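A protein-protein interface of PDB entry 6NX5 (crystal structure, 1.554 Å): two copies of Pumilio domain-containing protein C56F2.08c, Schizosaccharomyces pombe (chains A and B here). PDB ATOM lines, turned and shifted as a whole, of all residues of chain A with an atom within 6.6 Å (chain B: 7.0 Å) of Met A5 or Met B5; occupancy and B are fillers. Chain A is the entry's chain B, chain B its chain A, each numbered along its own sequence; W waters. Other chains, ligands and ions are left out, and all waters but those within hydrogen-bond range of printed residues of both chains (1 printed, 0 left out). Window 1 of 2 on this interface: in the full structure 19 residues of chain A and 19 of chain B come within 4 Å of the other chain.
The indole nitrogen (NE1) of Trp A34 sits at hydrogen-bond distance from the backbone carbonyl oxygen (O) of Gly B3.
O of Met B5 is in hydrogen-bond range of N of Ala B76. The backbone carbonyl oxygen (O) of Met B74 sits at hydrogen-bond distance from the backbone NH (N) of Tyr B7. The backbone NH (N) of Ile B43 sits at hydrogen-bond distance from the backbone carbonyl oxygen (O) of Trp B34. The backbone carbonyl oxygen (O) of Met A5 sits at hydrogen-bond distance from the backbone NH (N) of Ala A76. N of Tyr A7 lies within hydrogen-bond range of O of Met A74, at 2.8 Å. The backbone carbonyl oxygen (O) of Trp A34 lies within hydrogen-bond range of the backbone NH (N) of Ile A43.
CE of Met A5 touches CE of Met B5, at 3.8 Å. Tyr A7 touches Leu B36 (CB to CD2, 3.8 Å). Gly B2 touches Trp A34. CE2 of Trp A34 touches CG of Met B5 (3.4 Å). Trp A34 touches Ala B76 (CB to CB, 3.9 Å). Trp A34 touches Lys B77. Ala B76 touches Leu A36. Met A74 touches Leu B36. Leu A75 touches Leu B36. Ala A76 touches Leu B36 (CA to CD2, 3.7 Å).
Of the printed residues of chain B, Met A5 touches Met B5 (3.8 Å) and Trp B34 (3.6 Å). Of the printed residues of chain B, Met A74 touches Leu B36. Of the printed residues of chain B, Lys A77 touches Trp B34 (3.2 Å). Met B5 touches just these residues of chain A: Met A5, Trp A34 and Ile A43.
Printed residues of chain A that touch a printed residue of chain B: Met A5, Tyr A7, Trp A34, Leu A36, Ile A43, Met A74, Leu A75, Ala A76 and Lys A77. Printed residues of chain B that touch a printed residue of chain A: Gly B2, Gly B3, Met B5, Tyr B7, Trp B34, Leu B36, Met B74, Ala B76, Lys B77 and Ser B79. Hydrophobic or aromatic side chains of chain B that line the printed part of chain A: Met B5, Tyr B7, Trp B34, Leu B36 and Ala B76.
Tyr A7 touches Leu B36, and with the chains exchanged Leu A36 touches Tyr B7. Trp A34 touches Lys B77, and with the chains exchanged Lys A77 touches Trp B34. Leu A36 touches Met B74, and with the chains exchanged Met A74 touches Leu B36. Leu A36 touches Ala B76, and with the chains exchanged Ala A76 touches Leu B36. Positions printed for both chains: 3, 4, 5, 6, 7, 34, 36, 43, 44, 45, 46, 52, 74, 75, 76 and 77. Of the 19 pairs that touch across the chains among the printed residues, 14 have their exchanged pair printed and touching as well.
Water W1 lies within hydrogen-bond range of the side-chain hydroxyl (OH) of Tyr B7 (2.5 Å) and the side-chain sulfur (SD) of Met A74 (3.7 Å).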
ATOM      1  N   GLY A   3      29.606   3.483  -2.653  1.00  0.00           N
ATOM      2  CA  GLY A   3      29.410   4.648  -3.501  1.00  0.00           C
ATOM      3  C   GLY A   3      30.482   5.706  -3.363  1.00  0.00           C
ATOM      4  O   GLY A   3      31.578   5.445  -2.839  1.00  0.00           O
ATOM      5  N   SER A   4      30.186   6.903  -3.868  1.00  0.00           N
ATOM      6  CA  SER A   4      31.105   8.026  -3.707  1.00  0.00           C
ATOM      7  C   SER A   4      30.295   9.307  -3.586  1.00  0.00           C
ATOM      8  O   SER A   4      29.092   9.341  -3.867  1.00  0.00           O
ATOM      9  CB  SER A   4      32.105   8.098  -4.867  1.00  0.00           C
ATOM     10  OG  SER A   4      31.434   8.134  -6.124  1.00  0.00           O
ATOM     11  N   MET A   5      30.967  10.377  -3.194  1.00  0.00           N
ATOM     12  CA  MET A   5      30.256  11.610  -2.907  1.00  0.00           C
ATOM     13  C   MET A   5      31.144  12.793  -3.264  1.00  0.00           C
ATOM     14  O   MET A   5      32.371  12.714  -3.144  1.00  0.00           O
ATOM     15  CB  MET A   5      29.835  11.657  -1.440  1.00  0.00           C
ATOM     16  CG  MET A   5      29.548  13.050  -0.919  1.00  0.00           C
ATOM     17  SD  MET A   5      28.751  12.997   0.694  1.00  0.00           S
ATOM     18  CE  MET A   5      27.397  11.972   0.201  1.00  0.00           C
ATOM     19  N   LEU A   6      30.511  13.853  -3.765  1.00  0.00           N
ATOM     20  CA  LEU A   6      31.184  15.061  -4.221  1.00  0.00           C
ATOM     21  C   LEU A   6      30.563  16.270  -3.562  1.00  0.00           C
ATOM     22  O   LEU A   6      29.359  16.289  -3.294  1.00  0.00           O
ATOM     23  CB  LEU A   6      31.044  15.285  -5.727  1.00  0.00           C
ATOM     24  CG  LEU A   6      31.676  14.315  -6.695  1.00  0.00           C
ATOM     25  CD1 LEU A   6      31.256  14.677  -8.075  1.00  0.00           C
ATOM     26  CD2 LEU A   6      33.178  14.481  -6.556  1.00  0.00           C
ATOM     27  N   TYR A   7      31.381  17.300  -3.341  1.00  0.00           N
ATOM     28  CA  TYR A   7      30.889  18.615  -2.976  1.00  0.00           C
ATOM     29  C   TYR A   7      31.188  19.562  -4.122  1.00  0.00           C
ATOM     30  O   TYR A   7      32.350  19.722  -4.506  1.00  0.00           O
ATOM     31  CB  TYR A   7      31.529  19.110  -1.678  1.00  0.00           C
ATOM     32  CG  TYR A   7      31.129  20.527  -1.332  1.00  0.00           C
ATOM     33  CD1 TYR A   7      29.814  20.828  -0.991  1.00  0.00           C
ATOM     34  CD2 TYR A   7      32.054  21.547  -1.350  1.00  0.00           C
ATOM     35  CE1 TYR A   7      29.434  22.126  -0.686  1.00  0.00           C
ATOM     36  CE2 TYR A   7      31.681  22.841  -1.037  1.00  0.00           C
ATOM     37  CZ  TYR A   7      30.366  23.116  -0.712  1.00  0.00           C
ATOM     38  OH  TYR A   7      29.986  24.421  -0.401  1.00  0.00           O
ATOM     39  N   TRP A  34      21.817  17.026  -2.277  1.00  0.00           N
ATOM     40  CA  TRP A  34      21.444  18.019  -1.271  1.00  0.00           C
ATOM     41  C   TRP A  34      21.923  19.388  -1.742  1.00  0.00           C
ATOM     42  O   TRP A  34      23.124  19.574  -1.963  1.00  0.00           O
ATOM     43  CB  TRP A  34      22.070  17.712   0.090  1.00  0.00           C
ATOM     44  CG  TRP A  34      21.590  16.517   0.832  1.00  0.00           C
ATOM     45  CD1 TRP A  34      20.715  16.487   1.904  1.00  0.00           C
ATOM     46  CD2 TRP A  34      22.025  15.169   0.631  1.00  0.00           C
ATOM     47  NE1 TRP A  34      20.572  15.187   2.355  1.00  0.00           N
ATOM     48  CE2 TRP A  34      21.352  14.362   1.586  1.00  0.00           C
ATOM     49  CE3 TRP A  34      22.894  14.563  -0.283  1.00  0.00           C
ATOM     50  CZ2 TRP A  34      21.538  12.985   1.647  1.00  0.00           C
ATOM     51  CZ3 TRP A  34      23.086  13.183  -0.215  1.00  0.00           C
ATOM     52  CH2 TRP A  34      22.400  12.414   0.749  1.00  0.00           C
ATOM     53  N   LEU A  36      22.594  23.429  -1.053  1.00  0.00           N
ATOM     54  CA  LEU A  36      22.875  24.358   0.033  1.00  0.00           C
ATOM     55  C   LEU A  36      22.453  25.755  -0.399  1.00  0.00           C
ATOM     56  O   LEU A  36      22.778  26.182  -1.509  1.00  0.00           O
ATOM     57  CB  LEU A  36      24.358  24.317   0.408  1.00  0.00           C
ATOM     58  CG  LEU A  36      24.660  22.987   1.103  1.00  0.00           C
ATOM     59  CD1 LEU A  36      25.703  22.196   0.343  1.00  0.00           C
ATOM     60  CD2 LEU A  36      25.063  23.176   2.543  1.00  0.00           C
ATOM     61  N   ILE A  43      25.750  18.841  -2.600  1.00  0.00           N
ATOM     62  CA  ILE A  43      26.371  17.563  -2.260  1.00  0.00           C
ATOM     63  C   ILE A  43      25.735  16.517  -3.161  1.00  0.00           C
ATOM     64  O   ILE A  43      24.503  16.411  -3.196  1.00  0.00           O
ATOM     65  CB  ILE A  43      26.141  17.208  -0.782  1.00  0.00           C
ATOM     66  CG1 ILE A  43      26.782  18.277   0.103  1.00  0.00           C
ATOM     67  CG2 ILE A  43      26.710  15.830  -0.482  1.00  0.00           C
ATOM     68  CD1 ILE A  43      26.327  18.237   1.580  1.00  0.00           C
ATOM     69  N   VAL A  44      26.551  15.768  -3.891  1.00  0.00           N
ATOM     70  CA  VAL A  44      26.067  14.809  -4.887  1.00  0.00           C
ATOM     71  C   VAL A  44      26.566  13.421  -4.498  1.00  0.00           C
ATOM     72  O   VAL A  44      27.773  13.225  -4.344  1.00  0.00           O
ATOM     73  CB  VAL A  44      26.558  15.192  -6.302  1.00  0.00           C
ATOM     74  CG1 VAL A  44      26.144  14.100  -7.317  1.00  0.00           C
ATOM     75  CG2 VAL A  44      26.037  16.552  -6.675  1.00  0.00           C
ATOM     76  N   SER A  45      25.649  12.447  -4.377  1.00  0.00           N
ATOM     77  CA  SER A  45      25.980  11.067  -4.024  1.00  0.00           C
ATOM     78  C   SER A  45      25.817  10.140  -5.227  1.00  0.00           C
ATOM     79  O   SER A  45      24.766  10.155  -5.877  1.00  0.00           O
ATOM     80  CB  SER A  45      25.073  10.611  -2.875  1.00  0.00           C
ATOM     81  OG  SER A  45      25.194   9.229  -2.640  1.00  0.00           O
ATOM     82  N   TYR A  46      26.830   9.322  -5.503  1.00  0.00           N
ATOM     83  CA  TYR A  46      26.846   8.370  -6.605  1.00  0.00           C
ATOM     84  C   TYR A  46      26.787   6.933  -6.114  1.00  0.00           C
ATOM     85  O   TYR A  46      27.346   6.582  -5.072  1.00  0.00           O
ATOM     86  CB  TYR A  46      28.143   8.500  -7.394  1.00  0.00           C
ATOM     87  CG  TYR A  46      28.214   9.562  -8.452  1.00  0.00           C
ATOM     88  CD1 TYR A  46      29.179  10.568  -8.371  1.00  0.00           C
ATOM     89  CD2 TYR A  46      27.394   9.519  -9.576  1.00  0.00           C
ATOM     90  CE1 TYR A  46      29.298  11.519  -9.366  1.00  0.00           C
ATOM     91  CE2 TYR A  46      27.503  10.482 -10.590  1.00  0.00           C
ATOM     92  CZ  TYR A  46      28.472  11.472 -10.466  1.00  0.00           C
ATOM     93  OH  TYR A  46      28.599  12.418 -11.467  1.00  0.00           O
ATOM     94  N   SER A  48      28.430   4.329  -7.529  1.00  0.00           N
ATOM     95  CA  SER A  48      29.711   3.659  -7.710  1.00  0.00           C
ATOM     96  C   SER A  48      30.850   4.497  -7.173  1.00  0.00           C
ATOM     97  O   SER A  48      30.866   5.717  -7.365  1.00  0.00           O
ATOM     98  CB  SER A  48      29.994   3.396  -9.187  1.00  0.00           C
ATOM     99  OG  SER A  48      28.878   2.788  -9.803  1.00  0.00           O
ATOM    100  N   LEU A  49      31.833   3.815  -6.553  1.00  0.00           N
ATOM    101  CA  LEU A  49      33.034   4.474  -6.046  1.00  0.00           C
ATOM    102  C   LEU A  49      33.735   5.278  -7.130  1.00  0.00           C
ATOM    103  O   LEU A  49      34.199   6.394  -6.886  1.00  0.00           O
ATOM    104  CB  LEU A  49      33.980   3.418  -5.476  1.00  0.00           C
ATOM    105  CG  LEU A  49      35.283   3.855  -4.831  1.00  0.00           C
ATOM    106  CD1 LEU A  49      34.993   4.588  -3.536  1.00  0.00           C
ATOM    107  CD2 LEU A  49      36.115   2.611  -4.568  1.00  0.00           C
ATOM    108  N   ALA A  52      32.624   9.517  -8.683  1.00  0.00           N
ATOM    109  CA  ALA A  52      33.029  10.842  -8.230  1.00  0.00           C
ATOM    110  C   ALA A  52      34.366  11.244  -8.841  1.00  0.00           C
ATOM    111  O   ALA A  52      34.554  12.407  -9.210  1.00  0.00           O
ATOM    112  CB  ALA A  52      33.092  10.927  -6.703  1.00  0.00           C
ATOM    113  N   MET A  74      34.908  18.893  -5.442  1.00  0.00           N
ATOM    114  CA  MET A  74      35.779  18.299  -4.438  1.00  0.00           C
ATOM    115  C   MET A  74      35.299  16.901  -4.089  1.00  0.00           C
ATOM    116  O   MET A  74      34.119  16.711  -3.785  1.00  0.00           O
ATOM    117  CB  MET A  74      35.819  19.167  -3.181  1.00  0.00           C
ATOM    118  CG  MET A  74      36.327  20.563  -3.448  1.00  0.00           C
ATOM    119  SD  MET A  74      36.864  21.330  -1.920  1.00  0.00           S
ATOM    120  CE  MET A  74      38.327  20.347  -1.596  1.00  0.00           C
ATOM    121  N   LEU A  75      36.224  15.946  -4.058  1.00  0.00           N
ATOM    122  CA  LEU A  75      35.901  14.605  -3.589  1.00  0.00           C
ATOM    123  C   LEU A  75      35.693  14.621  -2.078  1.00  0.00           C
ATOM    124  O   LEU A  75      36.485  15.217  -1.339  1.00  0.00           O
ATOM    125  CB  LEU A  75      37.030  13.630  -3.946  1.00  0.00           C
ATOM    126  CG  LEU A  75      37.390  13.202  -5.369  1.00  0.00           C
ATOM    127  CD1 LEU A  75      38.363  12.032  -5.294  1.00  0.00           C
ATOM    128  CD2 LEU A  75      36.166  12.816  -6.186  1.00  0.00           C
ATOM    129  N   ALA A  76      34.633  13.966  -1.620  1.00  0.00           N
ATOM    130  CA  ALA A  76      34.318  13.844  -0.204  1.00  0.00           C
ATOM    131  C   ALA A  76      34.846  12.504   0.274  1.00  0.00           C
ATOM    132  O   ALA A  76      34.319  11.447  -0.106  1.00  0.00           O
ATOM    133  CB  ALA A  76      32.814  13.970   0.035  1.00  0.00           C
ATOM    134  N   LYS A  77      35.885  12.551   1.089  1.00  0.00           N
ATOM    135  CA  LYS A  77      36.590  11.348   1.494  1.00  0.00           C
ATOM    136  C   LYS A  77      35.860  10.688   2.656  1.00  0.00           C
ATOM    137  O   LYS A  77      35.767  11.286   3.737  1.00  0.00           O
ATOM    138  CB  LYS A  77      38.023  11.681   1.887  1.00  0.00           C
ATOM    139  CG  LYS A  77      38.870  10.463   2.211  1.00  0.00           C
ATOM    140  CD  LYS A  77      39.442   9.829   0.947  1.00  0.00           C
ATOM    141  CE  LYS A  77      40.522  10.706   0.321  1.00  0.00           C
ATOM    142  NZ  LYS A  77      41.172  10.038  -0.844  1.00  0.00           N
ATOM    143  N   GLY B   2      17.473  10.128   2.119  1.00  0.00           N
ATOM    144  CA  GLY B   2      17.008  11.006   3.177  1.00  0.00           C
ATOM    145  C   GLY B   2      18.124  11.380   4.132  1.00  0.00           C
ATOM    146  O   GLY B   2      19.311  11.116   3.909  1.00  0.00           O
ATOM    147  N   GLY B   3      17.713  12.029   5.218  1.00  0.00           N
ATOM    148  CA  GLY B   3      18.634  12.457   6.249  1.00  0.00           C
ATOM    149  C   GLY B   3      19.219  13.825   5.975  1.00  0.00           C
ATOM    150  O   GLY B   3      19.075  14.403   4.891  1.00  0.00           O
ATOM    151  N   SER B   4      19.858  14.371   7.001  1.00  0.00           N
ATOM    152  CA  SER B   4      20.294  15.760   6.973  1.00  0.00           C
ATOM    153  C   SER B   4      21.803  15.851   6.840  1.00  0.00           C
ATOM    154  O   SER B   4      22.539  15.078   7.463  1.00  0.00           O
ATOM    155  CB  SER B   4      19.808  16.492   8.223  1.00  0.00           C
ATOM    156  OG  SER B   4      18.390  16.493   8.233  1.00  0.00           O
ATOM    157  N   MET B   5      22.254  16.822   6.056  1.00  0.00           N
ATOM    158  CA  MET B   5      23.667  17.062   5.794  1.00  0.00           C
ATOM    159  C   MET B   5      24.062  18.449   6.270  1.00  0.00           C
ATOM    160  O   MET B   5      23.360  19.431   5.990  1.00  0.00           O
ATOM    161  CB  MET B   5      23.988  16.947   4.304  1.00  0.00           C
ATOM    162  CG  MET B   5      23.718  15.571   3.725  1.00  0.00           C
ATOM    163  SD  MET B   5      25.089  14.491   4.175  1.00  0.00           S
ATOM    164  CE  MET B   5      25.012  13.233   2.926  1.00  0.00           C
ATOM    165  N   LEU B   6      25.189  18.510   6.970  1.00  0.00           N
ATOM    166  CA  LEU B   6      25.828  19.766   7.366  1.00  0.00           C
ATOM    167  C   LEU B   6      27.141  19.894   6.624  1.00  0.00           C
ATOM    168  O   LEU B   6      27.945  18.949   6.614  1.00  0.00           O
ATOM    169  CB  LEU B   6      26.095  19.811   8.870  1.00  0.00           C
ATOM    170  CG  LEU B   6      24.894  19.658   9.804  1.00  0.00           C
ATOM    171  CD1 LEU B   6      25.360  19.627  11.242  1.00  0.00           C
ATOM    172  CD2 LEU B   6      23.871  20.763   9.624  1.00  0.00           C
ATOM    173  N   TYR B   7      27.355  21.054   6.014  1.00  0.00           N
ATOM    174  CA  TYR B   7      28.627  21.412   5.406  1.00  0.00           C
ATOM    175  C   TYR B   7      29.394  22.265   6.407  1.00  0.00           C
ATOM    176  O   TYR B   7      28.924  23.334   6.801  1.00  0.00           O
ATOM    177  CB  TYR B   7      28.409  22.155   4.084  1.00  0.00           C
ATOM    178  CG  TYR B   7      29.686  22.724   3.505  1.00  0.00           C
ATOM    179  CD1 TYR B   7      30.702  21.895   3.055  1.00  0.00           C
ATOM    180  CD2 TYR B   7      29.875  24.089   3.455  1.00  0.00           C
ATOM    181  CE1 TYR B   7      31.872  22.426   2.537  1.00  0.00           C
ATOM    182  CE2 TYR B   7      31.035  24.626   2.952  1.00  0.00           C
ATOM    183  CZ  TYR B   7      32.024  23.791   2.499  1.00  0.00           C
ATOM    184  OH  TYR B   7      33.171  24.346   1.989  1.00  0.00           O
ATOM    185  N   ASP B  32      27.368   9.739   9.482  1.00  0.00           N
ATOM    186  CA  ASP B  32      28.507   9.603   8.588  1.00  0.00           C
ATOM    187  C   ASP B  32      29.262  10.916   8.625  1.00  0.00           C
ATOM    188  O   ASP B  32      28.690  11.963   8.944  1.00  0.00           O
ATOM    189  CB  ASP B  32      28.073   9.289   7.152  1.00  0.00           C
ATOM    190  CG  ASP B  32      27.885   7.807   6.903  1.00  0.00           C
ATOM    191  OD1 ASP B  32      28.762   7.011   7.298  1.00  0.00           O
ATOM    192  OD2 ASP B  32      26.841   7.438   6.330  1.00  0.00           O
ATOM    193  N   TRP B  34      32.338  12.842   6.054  1.00  0.00           N
ATOM    194  CA  TRP B  34      33.257  12.877   4.923  1.00  0.00           C
ATOM    195  C   TRP B  34      34.181  14.078   5.067  1.00  0.00           C
ATOM    196  O   TRP B  34      33.741  15.170   5.436  1.00  0.00           O
ATOM    197  CB  TRP B  34      32.523  12.994   3.589  1.00  0.00           C
ATOM    198  CG  TRP B  34      31.596  11.873   3.275  1.00  0.00           C
ATOM    199  CD1 TRP B  34      31.852  10.819   2.461  1.00  0.00           C
ATOM    200  CD2 TRP B  34      30.254  11.716   3.737  1.00  0.00           C
ATOM    201  NE1 TRP B  34      30.752   9.996   2.392  1.00  0.00           N
ATOM    202  CE2 TRP B  34      29.757  10.524   3.172  1.00  0.00           C
ATOM    203  CE3 TRP B  34      29.424  12.459   4.578  1.00  0.00           C
ATOM    204  CZ2 TRP B  34      28.468  10.065   3.413  1.00  0.00           C
ATOM    205  CZ3 TRP B  34      28.130  12.002   4.810  1.00  0.00           C
ATOM    206  CH2 TRP B  34      27.671  10.813   4.233  1.00  0.00           C
ATOM    207  N   LEU B  36      36.725  16.829   3.273  1.00  0.00           N
ATOM    208  CA  LEU B  36      37.000  17.480   1.993  1.00  0.00           C
ATOM    209  C   LEU B  36      38.454  17.907   1.899  1.00  0.00           C
ATOM    210  O   LEU B  36      38.763  18.974   1.367  1.00  0.00           O
ATOM    211  CB  LEU B  36      36.076  18.672   1.785  1.00  0.00           C
ATOM    212  CG  LEU B  36      34.600  18.315   1.600  1.00  0.00           C
ATOM    213  CD1 LEU B  36      33.708  19.549   1.638  1.00  0.00           C
ATOM    214  CD2 LEU B  36      34.382  17.558   0.302  1.00  0.00           C
ATOM    215  N   ILE B  43      31.789  17.192   5.751  1.00  0.00           N
ATOM    216  CA  ILE B  43      30.348  16.981   5.668  1.00  0.00           C
ATOM    217  C   ILE B  43      29.962  16.025   6.778  1.00  0.00           C
ATOM    218  O   ILE B  43      30.612  14.986   6.965  1.00  0.00           O
ATOM    219  CB  ILE B  43      29.913  16.410   4.306  1.00  0.00           C
ATOM    220  CG1 ILE B  43      30.232  17.412   3.207  1.00  0.00           C
ATOM    221  CG2 ILE B  43      28.413  16.098   4.338  1.00  0.00           C
ATOM    222  CD1 ILE B  43      30.168  16.811   1.825  1.00  0.00           C
ATOM    223  N   VAL B  44      28.915  16.383   7.525  1.00  0.00           N
ATOM    224  CA  VAL B  44      28.456  15.611   8.671  1.00  0.00           C
ATOM    225  C   VAL B  44      26.984  15.318   8.462  1.00  0.00           C
ATOM    226  O   VAL B  44      26.211  16.229   8.140  1.00  0.00           O
ATOM    227  CB  VAL B  44      28.645  16.370   9.995  1.00  0.00           C
ATOM    228  CG1 VAL B  44      28.134  15.530  11.155  1.00  0.00           C
ATOM    229  CG2 VAL B  44      30.093  16.783  10.198  1.00  0.00           C
ATOM    230  N   SER B  45      26.587  14.060   8.636  1.00  0.00           N
ATOM    231  CA  SER B  45      25.197  13.671   8.458  1.00  0.00           C
ATOM    232  C   SER B  45      24.579  13.208   9.767  1.00  0.00           C
ATOM    233  O   SER B  45      25.227  12.533  10.577  1.00  0.00           O
ATOM    234  CB  SER B  45      25.050  12.564   7.404  1.00  0.00           C
ATOM    235  OG  SER B  45      25.561  11.335   7.877  1.00  0.00           O
ATOM    236  N   TYR B  46      23.318  13.590   9.956  1.00  0.00           N
ATOM    237  CA  TYR B  46      22.427  13.071  10.983  1.00  0.00           C
ATOM    238  C   TYR B  46      21.184  12.516  10.311  1.00  0.00           C
ATOM    239  O   TYR B  46      20.657  13.120   9.366  1.00  0.00           O
ATOM    240  CB  TYR B  46      21.963  14.150  11.949  1.00  0.00           C
ATOM    241  CG  TYR B  46      22.999  14.812  12.801  1.00  0.00           C
ATOM    242  CD1 TYR B  46      23.533  16.037  12.432  1.00  0.00           C
ATOM    243  CD2 TYR B  46      23.381  14.270  14.033  1.00  0.00           C
ATOM    244  CE1 TYR B  46      24.456  16.695  13.236  1.00  0.00           C
ATOM    245  CE2 TYR B  46      24.314  14.930  14.848  1.00  0.00           C
ATOM    246  CZ  TYR B  46      24.840  16.132  14.447  1.00  0.00           C
ATOM    247  OH  TYR B  46      25.755  16.788  15.238  1.00  0.00           O
ATOM    248  N   ALA B  52      20.290  17.892  13.416  1.00  0.00           N
ATOM    249  CA  ALA B  52      21.107  18.744  12.551  1.00  0.00           C
ATOM    250  C   ALA B  52      20.868  20.227  12.823  1.00  0.00           C
ATOM    251  O   ALA B  52      21.816  21.023  12.800  1.00  0.00           O
ATOM    252  CB  ALA B  52      20.841  18.425  11.074  1.00  0.00           C
ATOM    253  N   MET B  74      26.689  24.871   7.838  1.00  0.00           N
ATOM    254  CA  MET B  74      25.551  25.173   6.980  1.00  0.00           C
ATOM    255  C   MET B  74      24.705  23.921   6.829  1.00  0.00           C
ATOM    256  O   MET B  74      25.220  22.859   6.456  1.00  0.00           O
ATOM    257  CB  MET B  74      26.013  25.685   5.621  1.00  0.00           C
ATOM    258  CG  MET B  74      26.759  27.003   5.703  1.00  0.00           C
ATOM    259  SD  MET B  74      28.095  27.169   4.494  1.00  0.00           S
ATOM    260  CE  MET B  74      27.220  26.878   2.957  1.00  0.00           C
ATOM    261  N   LEU B  75      23.426  24.047   7.136  1.00  0.00           N
ATOM    262  CA  LEU B  75      22.489  22.944   6.969  1.00  0.00           C
ATOM    263  C   LEU B  75      21.964  22.940   5.540  1.00  0.00           C
ATOM    264  O   LEU B  75      21.340  23.915   5.100  1.00  0.00           O
ATOM    265  CB  LEU B  75      21.358  23.097   7.987  1.00  0.00           C
ATOM    266  CG  LEU B  75      20.147  22.198   7.844  1.00  0.00           C
ATOM    267  CD1 LEU B  75      20.547  20.736   7.963  1.00  0.00           C
ATOM    268  CD2 LEU B  75      19.151  22.584   8.932  1.00  0.00           C
ATOM    269  N   ALA B  76      22.171  21.828   4.829  1.00  0.00           N
ATOM    270  CA  ALA B  76      21.621  21.733   3.487  1.00  0.00           C
ATOM    271  C   ALA B  76      20.108  21.561   3.566  1.00  0.00           C
ATOM    272  O   ALA B  76      19.551  21.181   4.599  1.00  0.00           O
ATOM    273  CB  ALA B  76      22.230  20.551   2.718  1.00  0.00           C
ATOM    274  N   LYS B  77      19.438  21.856   2.454  1.00  0.00           N
ATOM    275  CA  LYS B  77      18.029  21.571   2.328  1.00  0.00           C
ATOM    276  C   LYS B  77      17.818  20.059   2.250  1.00  0.00           C
ATOM    277  O   LYS B  77      18.756  19.310   1.956  1.00  0.00           O
ATOM    278  CB  LYS B  77      17.473  22.240   1.068  1.00  0.00           C
ATOM    279  CG  LYS B  77      17.140  23.723   1.254  1.00  0.00           C
ATOM    280  CD  LYS B  77      16.593  24.297  -0.036  1.00  0.00           C
ATOM    281  CE  LYS B  77      17.725  24.629  -1.007  1.00  0.00           C
ATOM    282  NZ  LYS B  77      17.234  24.757  -2.404  1.00  0.00           N
ATOM    283  N   SER B  79      17.145  16.512   0.826  1.00  0.00           N
ATOM    284  CA  SER B  79      17.640  16.028  -0.441  1.00  0.00           C
ATOM    285  C   SER B  79      16.520  15.670  -1.420  1.00  0.00           C
ATOM    286  O   SER B  79      15.340  15.474  -1.061  1.00  0.00           O
ATOM    287  CB  SER B  79      18.506  14.804  -0.197  1.00  0.00           C
ATOM    288  OG  SER B  79      17.693  13.771   0.331  1.00  0.00           O
HETATM  289  O   HOH W   1      34.979  23.263   0.679  1.00  0.00           O
